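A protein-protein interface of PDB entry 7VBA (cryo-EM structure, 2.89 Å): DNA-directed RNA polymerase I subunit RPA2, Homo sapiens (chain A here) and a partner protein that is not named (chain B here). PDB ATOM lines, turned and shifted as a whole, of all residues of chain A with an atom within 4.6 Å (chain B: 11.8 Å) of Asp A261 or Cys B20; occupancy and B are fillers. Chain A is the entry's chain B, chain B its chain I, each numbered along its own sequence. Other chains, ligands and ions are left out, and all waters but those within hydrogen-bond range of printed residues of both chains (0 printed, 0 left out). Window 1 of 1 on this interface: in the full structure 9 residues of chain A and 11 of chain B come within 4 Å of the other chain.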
ATOM      1  N   LYS A 254      15.949  -1.227 -37.900  1.00  0.00           N
ATOM      2  CA  LYS A 254      16.061  -2.563 -37.258  1.00  0.00           C
ATOM      3  C   LYS A 254      16.517  -3.613 -38.259  1.00  0.00           C
ATOM      4  O   LYS A 254      17.235  -4.511 -37.850  1.00  0.00           O
ATOM      5  CB  LYS A 254      14.719  -2.974 -36.661  1.00  0.00           C
ATOM      6  CG  LYS A 254      14.375  -2.310 -35.336  1.00  0.00           C
ATOM      7  CD  LYS A 254      14.856  -3.083 -34.135  1.00  0.00           C
ATOM      8  CE  LYS A 254      13.822  -4.066 -33.635  1.00  0.00           C
ATOM      9  NZ  LYS A 254      12.610  -3.372 -33.141  1.00  0.00           N
ATOM     10  N   PHE A 259      21.234  -4.359 -33.899  1.00  0.00           N
ATOM     11  CA  PHE A 259      21.600  -3.635 -32.661  1.00  0.00           C
ATOM     12  C   PHE A 259      20.345  -3.565 -31.805  1.00  0.00           C
ATOM     13  O   PHE A 259      19.252  -3.765 -32.341  1.00  0.00           O
ATOM     14  CB  PHE A 259      21.940  -2.174 -32.942  1.00  0.00           C
ATOM     15  CG  PHE A 259      23.306  -1.826 -33.467  1.00  0.00           C
ATOM     16  CD1 PHE A 259      24.316  -2.766 -33.542  1.00  0.00           C
ATOM     17  CD2 PHE A 259      23.582  -0.524 -33.855  1.00  0.00           C
ATOM     18  CE1 PHE A 259      25.570  -2.412 -34.015  1.00  0.00           C
ATOM     19  CE2 PHE A 259      24.835  -0.171 -34.325  1.00  0.00           C
ATOM     20  CZ  PHE A 259      25.827  -1.118 -34.405  1.00  0.00           C
ATOM     21  N   SER A 260      20.503  -3.205 -30.543  1.00  0.00           N
ATOM     22  CA  SER A 260      19.386  -3.145 -29.589  1.00  0.00           C
ATOM     23  C   SER A 260      18.563  -1.925 -29.947  1.00  0.00           C
ATOM     24  O   SER A 260      19.065  -1.115 -30.713  1.00  0.00           O
ATOM     25  CB  SER A 260      19.984  -2.986 -28.276  1.00  0.00           C
ATOM     26  OG  SER A 260      21.376  -2.774 -28.415  1.00  0.00           O
ATOM     27  N   ASP A 261      17.346  -1.789 -29.437  1.00  0.00           N
ATOM     28  CA  ASP A 261      16.592  -0.549 -29.716  1.00  0.00           C
ATOM     29  C   ASP A 261      17.165   0.626 -28.933  1.00  0.00           C
ATOM     30  O   ASP A 261      16.915   1.725 -29.357  1.00  0.00           O
ATOM     31  CB  ASP A 261      15.111  -0.746 -29.463  1.00  0.00           C
ATOM     32  CG  ASP A 261      14.351  -1.173 -30.701  1.00  0.00           C
ATOM     33  OD1 ASP A 261      14.873  -0.941 -31.800  1.00  0.00           O
ATOM     34  OD2 ASP A 261      13.244  -1.732 -30.555  1.00  0.00           O
ATOM     35  N   TYR A 262      17.898   0.416 -27.848  1.00  0.00           N
ATOM     36  CA  TYR A 262      18.527   1.548 -27.147  1.00  0.00           C
ATOM     37  C   TYR A 262      19.709   2.052 -27.931  1.00  0.00           C
ATOM     38  O   TYR A 262      19.855   3.250 -28.005  1.00  0.00           O
ATOM     39  CB  TYR A 262      19.173   1.156 -25.836  1.00  0.00           C
ATOM     40  CG  TYR A 262      19.646   2.313 -24.997  1.00  0.00           C
ATOM     41  CD1 TYR A 262      18.848   3.416 -24.768  1.00  0.00           C
ATOM     42  CD2 TYR A 262      20.897   2.300 -24.420  1.00  0.00           C
ATOM     43  CE1 TYR A 262      19.284   4.474 -23.987  1.00  0.00           C
ATOM     44  CE2 TYR A 262      21.352   3.342 -23.635  1.00  0.00           C
ATOM     45  CZ  TYR A 262      20.542   4.434 -23.418  1.00  0.00           C
ATOM     46  OH  TYR A 262      21.005   5.455 -22.643  1.00  0.00           O
ATOM     47  N   GLN A 263      20.532   1.180 -28.485  1.00  0.00           N
ATOM     48  CA  GLN A 263      21.663   1.642 -29.333  1.00  0.00           C
ATOM     49  C   GLN A 263      21.175   2.353 -30.599  1.00  0.00           C
ATOM     50  O   GLN A 263      21.744   3.383 -30.918  1.00  0.00           O
ATOM     51  CB  GLN A 263      22.660   0.525 -29.584  1.00  0.00           C
ATOM     52  CG  GLN A 263      24.020   1.019 -30.031  1.00  0.00           C
ATOM     53  CD  GLN A 263      24.800  -0.138 -30.595  1.00  0.00           C
ATOM     54  OE1 GLN A 263      24.307  -1.258 -30.661  1.00  0.00           O
ATOM     55  NE2 GLN A 263      26.033   0.123 -30.991  1.00  0.00           N
ATOM     56  N   ILE A 264      20.148   1.867 -31.277  1.00  0.00           N
ATOM     57  CA  ILE A 264      19.591   2.642 -32.418  1.00  0.00           C
ATOM     58  C   ILE A 264      19.185   4.028 -31.903  1.00  0.00           C
ATOM     59  O   ILE A 264      19.492   4.997 -32.568  1.00  0.00           O
ATOM     60  CB  ILE A 264      18.413   1.890 -33.049  1.00  0.00           C
ATOM     61  CG1 ILE A 264      18.876   0.625 -33.767  1.00  0.00           C
ATOM     62  CG2 ILE A 264      17.617   2.794 -33.970  1.00  0.00           C
ATOM     63  CD1 ILE A 264      17.744  -0.221 -34.276  1.00  0.00           C
ATOM     64  N   PHE A 265      18.563   4.132 -30.732  1.00  0.00           N
ATOM     65  CA  PHE A 265      18.068   5.402 -30.139  1.00  0.00           C
ATOM     66  C   PHE A 265      19.221   6.294 -29.751  1.00  0.00           C
ATOM     67  O   PHE A 265      19.200   7.453 -30.069  1.00  0.00           O
ATOM     68  CB  PHE A 265      17.313   5.052 -28.861  1.00  0.00           C
ATOM     69  CG  PHE A 265      17.024   6.124 -27.844  1.00  0.00           C
ATOM     70  CD1 PHE A 265      15.819   6.798 -27.855  1.00  0.00           C
ATOM     71  CD2 PHE A 265      17.906   6.382 -26.812  1.00  0.00           C
ATOM     72  CE1 PHE A 265      15.535   7.759 -26.904  1.00  0.00           C
ATOM     73  CE2 PHE A 265      17.623   7.343 -25.859  1.00  0.00           C
ATOM     74  CZ  PHE A 265      16.436   8.026 -25.907  1.00  0.00           C
ATOM     75  N   LEU A 286      10.588   3.303 -32.653  1.00  0.00           N
ATOM     76  CA  LEU A 286      11.084   1.942 -32.342  1.00  0.00           C
ATOM     77  C   LEU A 286       9.985   1.029 -31.784  1.00  0.00           C
ATOM     78  O   LEU A 286       9.978  -0.148 -32.125  1.00  0.00           O
ATOM     79  CB  LEU A 286      12.282   2.064 -31.399  1.00  0.00           C
ATOM     80  CG  LEU A 286      13.411   2.927 -31.931  1.00  0.00           C
ATOM     81  CD1 LEU A 286      14.479   3.120 -30.878  1.00  0.00           C
ATOM     82  CD2 LEU A 286      13.987   2.309 -33.189  1.00  0.00           C
ATOM     83  N   ARG A 287       9.112   1.530 -30.930  1.00  0.00           N
ATOM     84  CA  ARG A 287       8.139   0.640 -30.267  1.00  0.00           C
ATOM     85  C   ARG A 287       6.823   0.609 -30.998  1.00  0.00           C
ATOM     86  O   ARG A 287       6.321  -0.476 -31.258  1.00  0.00           O
ATOM     87  CB  ARG A 287       7.717   1.266 -28.942  1.00  0.00           C
ATOM     88  CG  ARG A 287       6.432   0.714 -28.342  1.00  0.00           C
ATOM     89  CD  ARG A 287       6.026   1.437 -27.075  1.00  0.00           C
ATOM     90  NE  ARG A 287       6.107   2.886 -27.163  1.00  0.00           N
ATOM     91  CZ  ARG A 287       6.880   3.639 -26.395  1.00  0.00           C
ATOM     92  NH1 ARG A 287       7.642   3.081 -25.474  1.00  0.00           N
ATOM     93  NH2 ARG A 287       6.885   4.948 -26.543  1.00  0.00           N
ATOM     94  N   GLU A 291       7.765  -3.098 -32.042  1.00  0.00           N
ATOM     95  CA  GLU A 291       7.499  -4.019 -30.915  1.00  0.00           C
ATOM     96  C   GLU A 291       6.103  -4.554 -31.198  1.00  0.00           C
ATOM     97  O   GLU A 291       5.627  -5.400 -30.442  1.00  0.00           O
ATOM     98  CB  GLU A 291       7.638  -3.321 -29.572  1.00  0.00           C
ATOM     99  CG  GLU A 291       8.017  -4.258 -28.449  1.00  0.00           C
ATOM    100  CD  GLU A 291       7.940  -3.604 -27.085  1.00  0.00           C
ATOM    101  OE1 GLU A 291       8.308  -4.263 -26.102  1.00  0.00           O
ATOM    102  OE2 GLU A 291       7.513  -2.436 -27.017  1.00  0.00           O
ATOM    103  N   THR B   9      20.275   2.741 -18.732  1.00  0.00           N
ATOM    104  CA  THR B   9      19.325   3.152 -19.755  1.00  0.00           C
ATOM    105  C   THR B   9      17.987   3.475 -19.099  1.00  0.00           C
ATOM    106  O   THR B   9      17.510   2.750 -18.223  1.00  0.00           O
ATOM    107  CB  THR B   9      19.162   2.058 -20.810  1.00  0.00           C
ATOM    108  OG1 THR B   9      18.299   2.524 -21.854  1.00  0.00           O
ATOM    109  CG2 THR B   9      18.574   0.818 -20.197  1.00  0.00           C
ATOM    110  N   CYS B  10      17.376   4.575 -19.532  1.00  0.00           N
ATOM    111  CA  CYS B  10      16.402   5.290 -18.718  1.00  0.00           C
ATOM    112  C   CYS B  10      14.972   5.057 -19.184  1.00  0.00           C
ATOM    113  O   CYS B  10      14.571   5.540 -20.247  1.00  0.00           O
ATOM    114  CB  CYS B  10      16.702   6.791 -18.720  1.00  0.00           C
ATOM    115  SG  CYS B  10      18.242   7.244 -17.897  1.00  0.00           S
ATOM    116  N   SER B  11      14.216   4.304 -18.386  1.00  0.00           N
ATOM    117  CA  SER B  11      12.766   4.445 -18.291  1.00  0.00           C
ATOM    118  C   SER B  11      11.984   3.951 -19.502  1.00  0.00           C
ATOM    119  O   SER B  11      10.750   3.916 -19.465  1.00  0.00           O
ATOM    120  CB  SER B  11      12.413   5.910 -18.027  1.00  0.00           C
ATOM    121  OG  SER B  11      13.149   6.417 -16.929  1.00  0.00           O
ATOM    122  N   SER B  12      12.665   3.563 -20.574  1.00  0.00           N
ATOM    123  CA  SER B  12      11.982   3.066 -21.759  1.00  0.00           C
ATOM    124  C   SER B  12      12.690   1.879 -22.394  1.00  0.00           C
ATOM    125  O   SER B  12      12.285   1.436 -23.473  1.00  0.00           O
ATOM    126  CB  SER B  12      11.819   4.188 -22.784  1.00  0.00           C
ATOM    127  OG  SER B  12      10.907   3.813 -23.800  1.00  0.00           O
ATOM    128  N   PHE B  13      13.724   1.347 -21.748  1.00  0.00           N
ATOM    129  CA  PHE B  13      14.483   0.230 -22.283  1.00  0.00           C
ATOM    130  C   PHE B  13      14.837  -0.728 -21.152  1.00  0.00           C
ATOM    131  O   PHE B  13      15.039  -0.313 -20.008  1.00  0.00           O
ATOM    132  CB  PHE B  13      15.730   0.736 -23.021  1.00  0.00           C
ATOM    133  CG  PHE B  13      15.410   1.699 -24.134  1.00  0.00           C
ATOM    134  CD1 PHE B  13      14.923   1.241 -25.344  1.00  0.00           C
ATOM    135  CD2 PHE B  13      15.565   3.062 -23.960  1.00  0.00           C
ATOM    136  CE1 PHE B  13      14.615   2.121 -26.359  1.00  0.00           C
ATOM    137  CE2 PHE B  13      15.258   3.942 -24.975  1.00  0.00           C
ATOM    138  CZ  PHE B  13      14.781   3.470 -26.173  1.00  0.00           C
ATOM    139  N   GLN B  14      14.910  -2.019 -21.490  1.00  0.00           N
ATOM    140  CA  GLN B  14      14.931  -3.068 -20.471  1.00  0.00           C
ATOM    141  C   GLN B  14      16.070  -2.882 -19.472  1.00  0.00           C
ATOM    142  O   GLN B  14      15.937  -3.245 -18.299  1.00  0.00           O
ATOM    143  CB  GLN B  14      15.006  -4.438 -21.147  1.00  0.00           C
ATOM    144  CG  GLN B  14      13.643  -5.097 -21.323  1.00  0.00           C
ATOM    145  CD  GLN B  14      13.592  -6.076 -22.480  1.00  0.00           C
ATOM    146  OE1 GLN B  14      14.318  -5.935 -23.462  1.00  0.00           O
ATOM    147  NE2 GLN B  14      12.725  -7.071 -22.373  1.00  0.00           N
ATOM    148  N   SER B  15      17.196  -2.327 -19.915  1.00  0.00           N
ATOM    149  CA  SER B  15      18.295  -1.954 -19.025  1.00  0.00           C
ATOM    150  C   SER B  15      19.096  -3.147 -18.520  1.00  0.00           C
ATOM    151  O   SER B  15      20.143  -2.977 -17.887  1.00  0.00           O
ATOM    152  CB  SER B  15      17.764  -1.162 -17.831  1.00  0.00           C
ATOM    153  OG  SER B  15      18.776  -0.994 -16.854  1.00  0.00           O
ATOM    154  N   ASP B  16      18.610  -4.356 -18.792  1.00  0.00           N
ATOM    155  CA  ASP B  16      19.413  -5.563 -18.698  1.00  0.00           C
ATOM    156  C   ASP B  16      19.282  -6.412 -19.946  1.00  0.00           C
ATOM    157  O   ASP B  16      20.205  -7.161 -20.277  1.00  0.00           O
ATOM    158  CB  ASP B  16      18.999  -6.389 -17.471  1.00  0.00           C
ATOM    159  CG  ASP B  16      19.974  -7.506 -17.152  1.00  0.00           C
ATOM    160  OD1 ASP B  16      20.960  -7.679 -17.902  1.00  0.00           O
ATOM    161  OD2 ASP B  16      19.757  -8.207 -16.145  1.00  0.00           O
ATOM    162  N   LEU B  17      18.195  -6.253 -20.659  1.00  0.00           N
ATOM    163  CA  LEU B  17      18.079  -7.000 -21.919  1.00  0.00           C
ATOM    164  C   LEU B  17      18.506  -6.019 -22.966  1.00  0.00           C
ATOM    165  O   LEU B  17      19.678  -5.650 -22.933  1.00  0.00           O
ATOM    166  CB  LEU B  17      16.625  -7.420 -21.950  1.00  0.00           C
ATOM    167  CG  LEU B  17      16.316  -8.067 -20.602  1.00  0.00           C
ATOM    168  CD1 LEU B  17      14.869  -8.000 -20.228  1.00  0.00           C
ATOM    169  CD2 LEU B  17      16.868  -9.476 -20.484  1.00  0.00           C
ATOM    170  N   ASP B  18      17.585  -5.521 -23.763  1.00  0.00           N
ATOM    171  CA  ASP B  18      18.025  -4.453 -24.689  1.00  0.00           C
ATOM    172  C   ASP B  18      16.834  -3.710 -25.247  1.00  0.00           C
ATOM    173  O   ASP B  18      16.897  -2.482 -25.238  1.00  0.00           O
ATOM    174  CB  ASP B  18      18.783  -5.057 -25.868  1.00  0.00           C
ATOM    175  CG  ASP B  18      18.117  -6.241 -26.551  1.00  0.00           C
ATOM    176  OD1 ASP B  18      17.444  -7.018 -25.848  1.00  0.00           O
ATOM    177  OD2 ASP B  18      18.280  -6.372 -27.782  1.00  0.00           O
ATOM    178  N   PHE B  19      15.845  -4.460 -25.759  1.00  0.00           N
ATOM    179  CA  PHE B  19      14.720  -3.818 -26.423  1.00  0.00           C
ATOM    180  C   PHE B  19      14.095  -2.745 -25.534  1.00  0.00           C
ATOM    181  O   PHE B  19      14.515  -2.505 -24.399  1.00  0.00           O
ATOM    182  CB  PHE B  19      13.685  -4.867 -26.820  1.00  0.00           C
ATOM    183  CG  PHE B  19      14.290  -6.175 -27.250  1.00  0.00           C
ATOM    184  CD1 PHE B  19      14.895  -6.297 -28.490  1.00  0.00           C
ATOM    185  CD2 PHE B  19      14.277  -7.272 -26.405  1.00  0.00           C
ATOM    186  CE1 PHE B  19      15.458  -7.496 -28.887  1.00  0.00           C
ATOM    187  CE2 PHE B  19      14.841  -8.472 -26.797  1.00  0.00           C
ATOM    188  CZ  PHE B  19      15.431  -8.583 -28.039  1.00  0.00           C
ATOM    189  N   CYS B  20      13.082  -2.078 -26.079  1.00  0.00           N
ATOM    190  CA  CYS B  20      12.356  -1.035 -25.373  1.00  0.00           C
ATOM    191  C   CYS B  20      11.060  -1.584 -24.791  1.00  0.00           C
ATOM    192  O   CYS B  20      10.366  -2.386 -25.418  1.00  0.00           O
ATOM    193  CB  CYS B  20      12.048   0.134 -26.307  1.00  0.00           C
ATOM    194  SG  CYS B  20      10.954  -0.275 -27.674  1.00  0.00           S
ATOM    195  N   SER B  21      10.729  -1.122 -23.589  1.00  0.00           N
ATOM    196  CA  SER B  21       9.532  -1.574 -22.897  1.00  0.00           C
ATOM    197  C   SER B  21       8.307  -0.924 -23.536  1.00  0.00           C
ATOM    198  O   SER B  21       8.398  -0.240 -24.559  1.00  0.00           O
ATOM    199  CB  SER B  21       9.635  -1.255 -21.409  1.00  0.00           C
ATOM    200  OG  SER B  21      10.712  -1.953 -20.813  1.00  0.00           O
ATOM    201  N   ASP B  22       7.132  -1.289 -23.020  1.00  0.00           N
ATOM    202  CA  ASP B  22       5.868  -0.731 -23.563  1.00  0.00           C
ATOM    203  C   ASP B  22       5.320   0.316 -22.587  1.00  0.00           C
ATOM    204  O   ASP B  22       5.947   0.523 -21.546  1.00  0.00           O
ATOM    205  CB  ASP B  22       4.882  -1.855 -23.866  1.00  0.00           C
ATOM    206  CG  ASP B  22       3.972  -1.569 -25.047  1.00  0.00           C
ATOM    207  OD1 ASP B  22       3.577  -0.399 -25.215  1.00  0.00           O
ATOM    208  OD2 ASP B  22       3.671  -2.519 -25.797  1.00  0.00           O
ATOM    209  N   CYS B  23       4.207   0.977 -22.915  1.00  0.00           N
ATOM    210  CA  CYS B  23       3.644   2.050 -22.044  1.00  0.00           C
ATOM    211  C   CYS B  23       2.958   1.474 -20.789  1.00  0.00           C
ATOM    212  O   CYS B  23       2.408   0.359 -20.887  1.00  0.00           O
ATOM    213  CB  CYS B  23       2.723   2.953 -22.851  1.00  0.00           C
ATOM    214  SG  CYS B  23       3.601   4.267 -23.737  1.00  0.00           S
ATOM    215  N   GLY B  24       2.952   2.208 -19.663  1.00  0.00           N
ATOM    216  CA  GLY B  24       2.426   1.672 -18.388  1.00  0.00           C
ATOM    217  C   GLY B  24       0.916   1.478 -18.292  1.00  0.00           C
ATOM    218  O   GLY B  24       0.195   2.407 -18.684  1.00  0.00           O
ATOM    219  N   LEU B  29       6.545  -3.305 -14.022  1.00  0.00           N
ATOM    220  CA  LEU B  29       7.264  -2.793 -15.207  1.00  0.00           C
ATOM    221  C   LEU B  29       6.761  -3.680 -16.325  1.00  0.00           C
ATOM    222  O   LEU B  29       6.798  -4.907 -16.168  1.00  0.00           O
ATOM    223  CB  LEU B  29       8.761  -3.035 -15.007  1.00  0.00           C
ATOM    224  CG  LEU B  29       9.630  -2.750 -16.231  1.00  0.00           C
ATOM    225  CD1 LEU B  29      10.325  -1.403 -16.107  1.00  0.00           C
ATOM    226  CD2 LEU B  29      10.646  -3.858 -16.450  1.00  0.00           C
ATOM    227  N   PRO B  30       6.359  -3.130 -17.476  1.00  0.00           N
ATOM    228  CA  PRO B  30       5.711  -3.952 -18.469  1.00  0.00           C
ATOM    229  C   PRO B  30       6.703  -4.815 -19.249  1.00  0.00           C
ATOM    230  O   PRO B  30       7.080  -4.421 -20.326  1.00  0.00           O
ATOM    231  CB  PRO B  30       5.079  -2.893 -19.391  1.00  0.00           C
ATOM    232  CG  PRO B  30       5.194  -1.577 -18.648  1.00  0.00           C
ATOM    233  CD  PRO B  30       6.458  -1.721 -17.835  1.00  0.00           C
ATOM    234  N   GLY B  31       7.061  -5.970 -18.693  1.00  0.00           N
ATOM    235  CA  GLY B  31       7.979  -6.883 -19.389  1.00  0.00           C
ATOM    236  C   GLY B  31       7.802  -6.820 -20.891  1.00  0.00           C
ATOM    237  O   GLY B  31       6.650  -6.966 -21.353  1.00  0.00           O
ATOM    238  N   ALA B  32       8.891  -6.666 -21.634  1.00  0.00           N
ATOM    239  CA  ALA B  32       8.859  -6.563 -23.081  1.00  0.00           C
ATOM    240  C   ALA B  32       8.504  -7.909 -23.703  1.00  0.00           C
ATOM    241  O   ALA B  32       8.630  -8.967 -23.081  1.00  0.00           O
ATOM    242  CB  ALA B  32      10.199  -6.067 -23.621  1.00  0.00           C
ATOM    243  N   GLN B  33       8.052  -7.853 -24.957  1.00  0.00           N
ATOM    244  CA  GLN B  33       7.670  -9.067 -25.670  1.00  0.00           C
ATOM    245  C   GLN B  33       8.796 -10.094 -25.679  1.00  0.00           C
ATOM    246  O   GLN B  33       8.556 -11.289 -25.886  1.00  0.00           O
ATOM    247  CB  GLN B  33       7.244  -8.714 -27.093  1.00  0.00           C
ATOM    248  CG  GLN B  33       8.398  -8.487 -28.051  1.00  0.00           C
ATOM    249  CD  GLN B  33       7.988  -8.628 -29.503  1.00  0.00           C
ATOM    250  OE1 GLN B  33       6.995  -8.044 -29.939  1.00  0.00           O
ATOM    251  NE2 GLN B  33       8.754  -9.402 -30.261  1.00  0.00           N
ATOM    252  N   ASP B  34      10.032  -9.652 -25.464  1.00  0.00           N
ATOM    253  CA  ASP B  34      11.193 -10.531 -25.422  1.00  0.00           C
ATOM    254  C   ASP B  34      11.870 -10.372 -24.069  1.00  0.00           C
ATOM    255  O   ASP B  34      12.146  -9.245 -23.644  1.00  0.00           O
ATOM    256  CB  ASP B  34      12.170 -10.190 -26.546  1.00  0.00           C
ATOM    257  CG  ASP B  34      11.521 -10.223 -27.913  1.00  0.00           C
ATOM    258  OD1 ASP B  34      10.345 -10.627 -28.009  1.00  0.00           O
ATOM    259  OD2 ASP B  34      12.197  -9.852 -28.896  1.00  0.00           O
ATOM    260  N   THR B  35      12.160 -11.493 -23.404  1.00  0.00           N
ATOM    261  CA  THR B  35      12.875 -11.422 -22.135  1.00  0.00           C
ATOM    262  C   THR B  35      12.093 -10.597 -21.118  1.00  0.00           C
ATOM    263  O   THR B  35      12.432  -9.441 -20.856  1.00  0.00           O
ATOM    264  CB  THR B  35      14.273 -10.839 -22.338  1.00  0.00           C
ATOM    265  OG1 THR B  35      14.170  -9.521 -22.886  1.00  0.00           O
ATOM    266  CG2 THR B  35      15.079 -11.707 -23.286  1.00  0.00           C
ATOM    267  N   VAL B  36      11.039 -11.173 -20.549  1.00  0.00           N
ATOM    268  CA  VAL B  36      10.018 -10.405 -19.845  1.00  0.00           C
ATOM    269  C   VAL B  36      10.433  -9.996 -18.437  1.00  0.00           C
ATOM    270  O   VAL B  36       9.585  -9.491 -17.687  1.00  0.00           O
ATOM    271  CB  VAL B  36       8.681 -11.177 -19.801  1.00  0.00           C
ATOM    272  CG1 VAL B  36       7.550 -10.295 -19.287  1.00  0.00           C
ATOM    273  CG2 VAL B  36       8.354 -11.731 -21.175  1.00  0.00           C
ATOM    274  N   THR B  37      11.690 -10.197 -18.044  1.00  0.00           N
ATOM    275  CA  THR B  37      12.157  -9.810 -16.717  1.00  0.00           C
ATOM    276  C   THR B  37      11.645  -8.426 -16.337  1.00  0.00           C
ATOM    277  O   THR B  37      11.616  -7.513 -17.167  1.00  0.00           O
ATOM    278  CB  THR B  37      13.685  -9.822 -16.675  1.00  0.00           C
ATOM    279  OG1 THR B  37      14.191  -8.802 -17.544  1.00  0.00           O
ATOM    280  CG2 THR B  37      14.214 -11.176 -17.133  1.00  0.00           C
ATOM    281  N   CYS B  38      11.250  -8.274 -15.074  1.00  0.00           N
ATOM    282  CA  CYS B  38      10.579  -7.074 -14.592  1.00  0.00           C
ATOM    283  C   CYS B  38      11.310  -6.484 -13.394  1.00  0.00           C
ATOM    284  O   CYS B  38      11.911  -7.212 -12.598  1.00  0.00           O
ATOM    285  CB  CYS B  38       9.129  -7.379 -14.208  1.00  0.00           C
ATOM    286  SG  CYS B  38       8.073  -7.877 -15.582  1.00  0.00           S
ATOM    287  N   ILE B  39      11.246  -5.157 -13.267  1.00  0.00           N
ATOM    288  CA  ILE B  39      11.862  -4.442 -12.155  1.00  0.00           C
ATOM    289  C   ILE B  39      11.291  -3.031 -12.121  1.00  0.00           C
ATOM    290  O   ILE B  39      11.002  -2.437 -13.161  1.00  0.00           O
ATOM    291  CB  ILE B  39      13.403  -4.417 -12.283  1.00  0.00           C
ATOM    292  CG1 ILE B  39      14.052  -3.968 -10.972  1.00  0.00           C
ATOM    293  CG2 ILE B  39      13.824  -3.520 -13.432  1.00  0.00           C
ATOM    294  CD1 ILE B  39      13.885  -4.956  -9.841  1.00  0.00           C
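Ser A260 touches just one residue of chain B: Asp B18. No residue of chain B comes within 4 Å of Ile A264. No residue of chain B comes within 4 Å of Leu A286. Arg A287 touches four residues of chain B. Of chain B, only Cys B20, Ser B21, Ala B32 and Gln B33 come within 4 Å of Glu A291. Printed residues of chain A within 4 Å of Asp B18: Ser A260 (3.4 Å). Of the printed residues of chain A, Ser B12 touches Arg A287 (3.7 Å). Printed residues of chain A within 4 Å of Ala B32: Glu A291 (3.6 Å). Asp B16 touches none of the printed residues of chain A. Cys B23 touches none of the printed residues of chain A. The nearest residue of chain B that does not touch Asp A261 is Asp B18 (4.3 Å). The nearest residue of chain A that does not touch Cys B20 is Leu A286 (4.4 Å).
Of the 27 printed residues of chain B, 9 touch a printed residue of chain A. Hydrophobic or aromatic side chains of chain B within 4 Å of the printed part of chain A: Phe B13 and Ala B32.
The backbone carbonyl oxygen of Glu A291 lies close to the side-chain amide oxygen of Gln B33 (3.0 Å). OE1 of Glu A291 lies close to O of Cys B20 (2.9 Å). O of Ser B21 sits close to OE2 of Glu A291.
Ser A260 touches Asp B18. CE1 of Phe B13 touches O of Asp A261, 3.8 Å away. SG of Cys B20 touches OD2 of Asp A261, at 3.96 Å. CE1 of Tyr A262 touches OG1 of Thr B9, at 3.1 Å. Phe B13 touches Tyr A262 (CD2 to CD1, 3.4 Å). Arg A287 touches Ser B12 (NH1 to OG, 3.7 Å). Arg A287 touches Cys B20. NH1 of Arg A287 touches O of Ser B21, 3.5 Å away. CD of Arg A287 touches OD1 of Asp B22, 3.6 Å away. CB of Ala B32 touches OE1 of Glu A291 (3.6 Å).
NZ of Lys A254 lies within salt-bridge range of OD2 of Asp A261 (3.1 Å). The backbone carbonyl oxygen of Ser B12 lies within hydrogen-bond range of the backbone NH of Ser B21, at 3.0 Å. The backbone NH (N) of Asp B18 sits at hydrogen-bond distance from the side-chain amide oxygen (OE1) of Gln B14, at 3.3 Å. NE2 of Gln B33 sits close to OD1 of Asp B34, 3.0 Å away.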
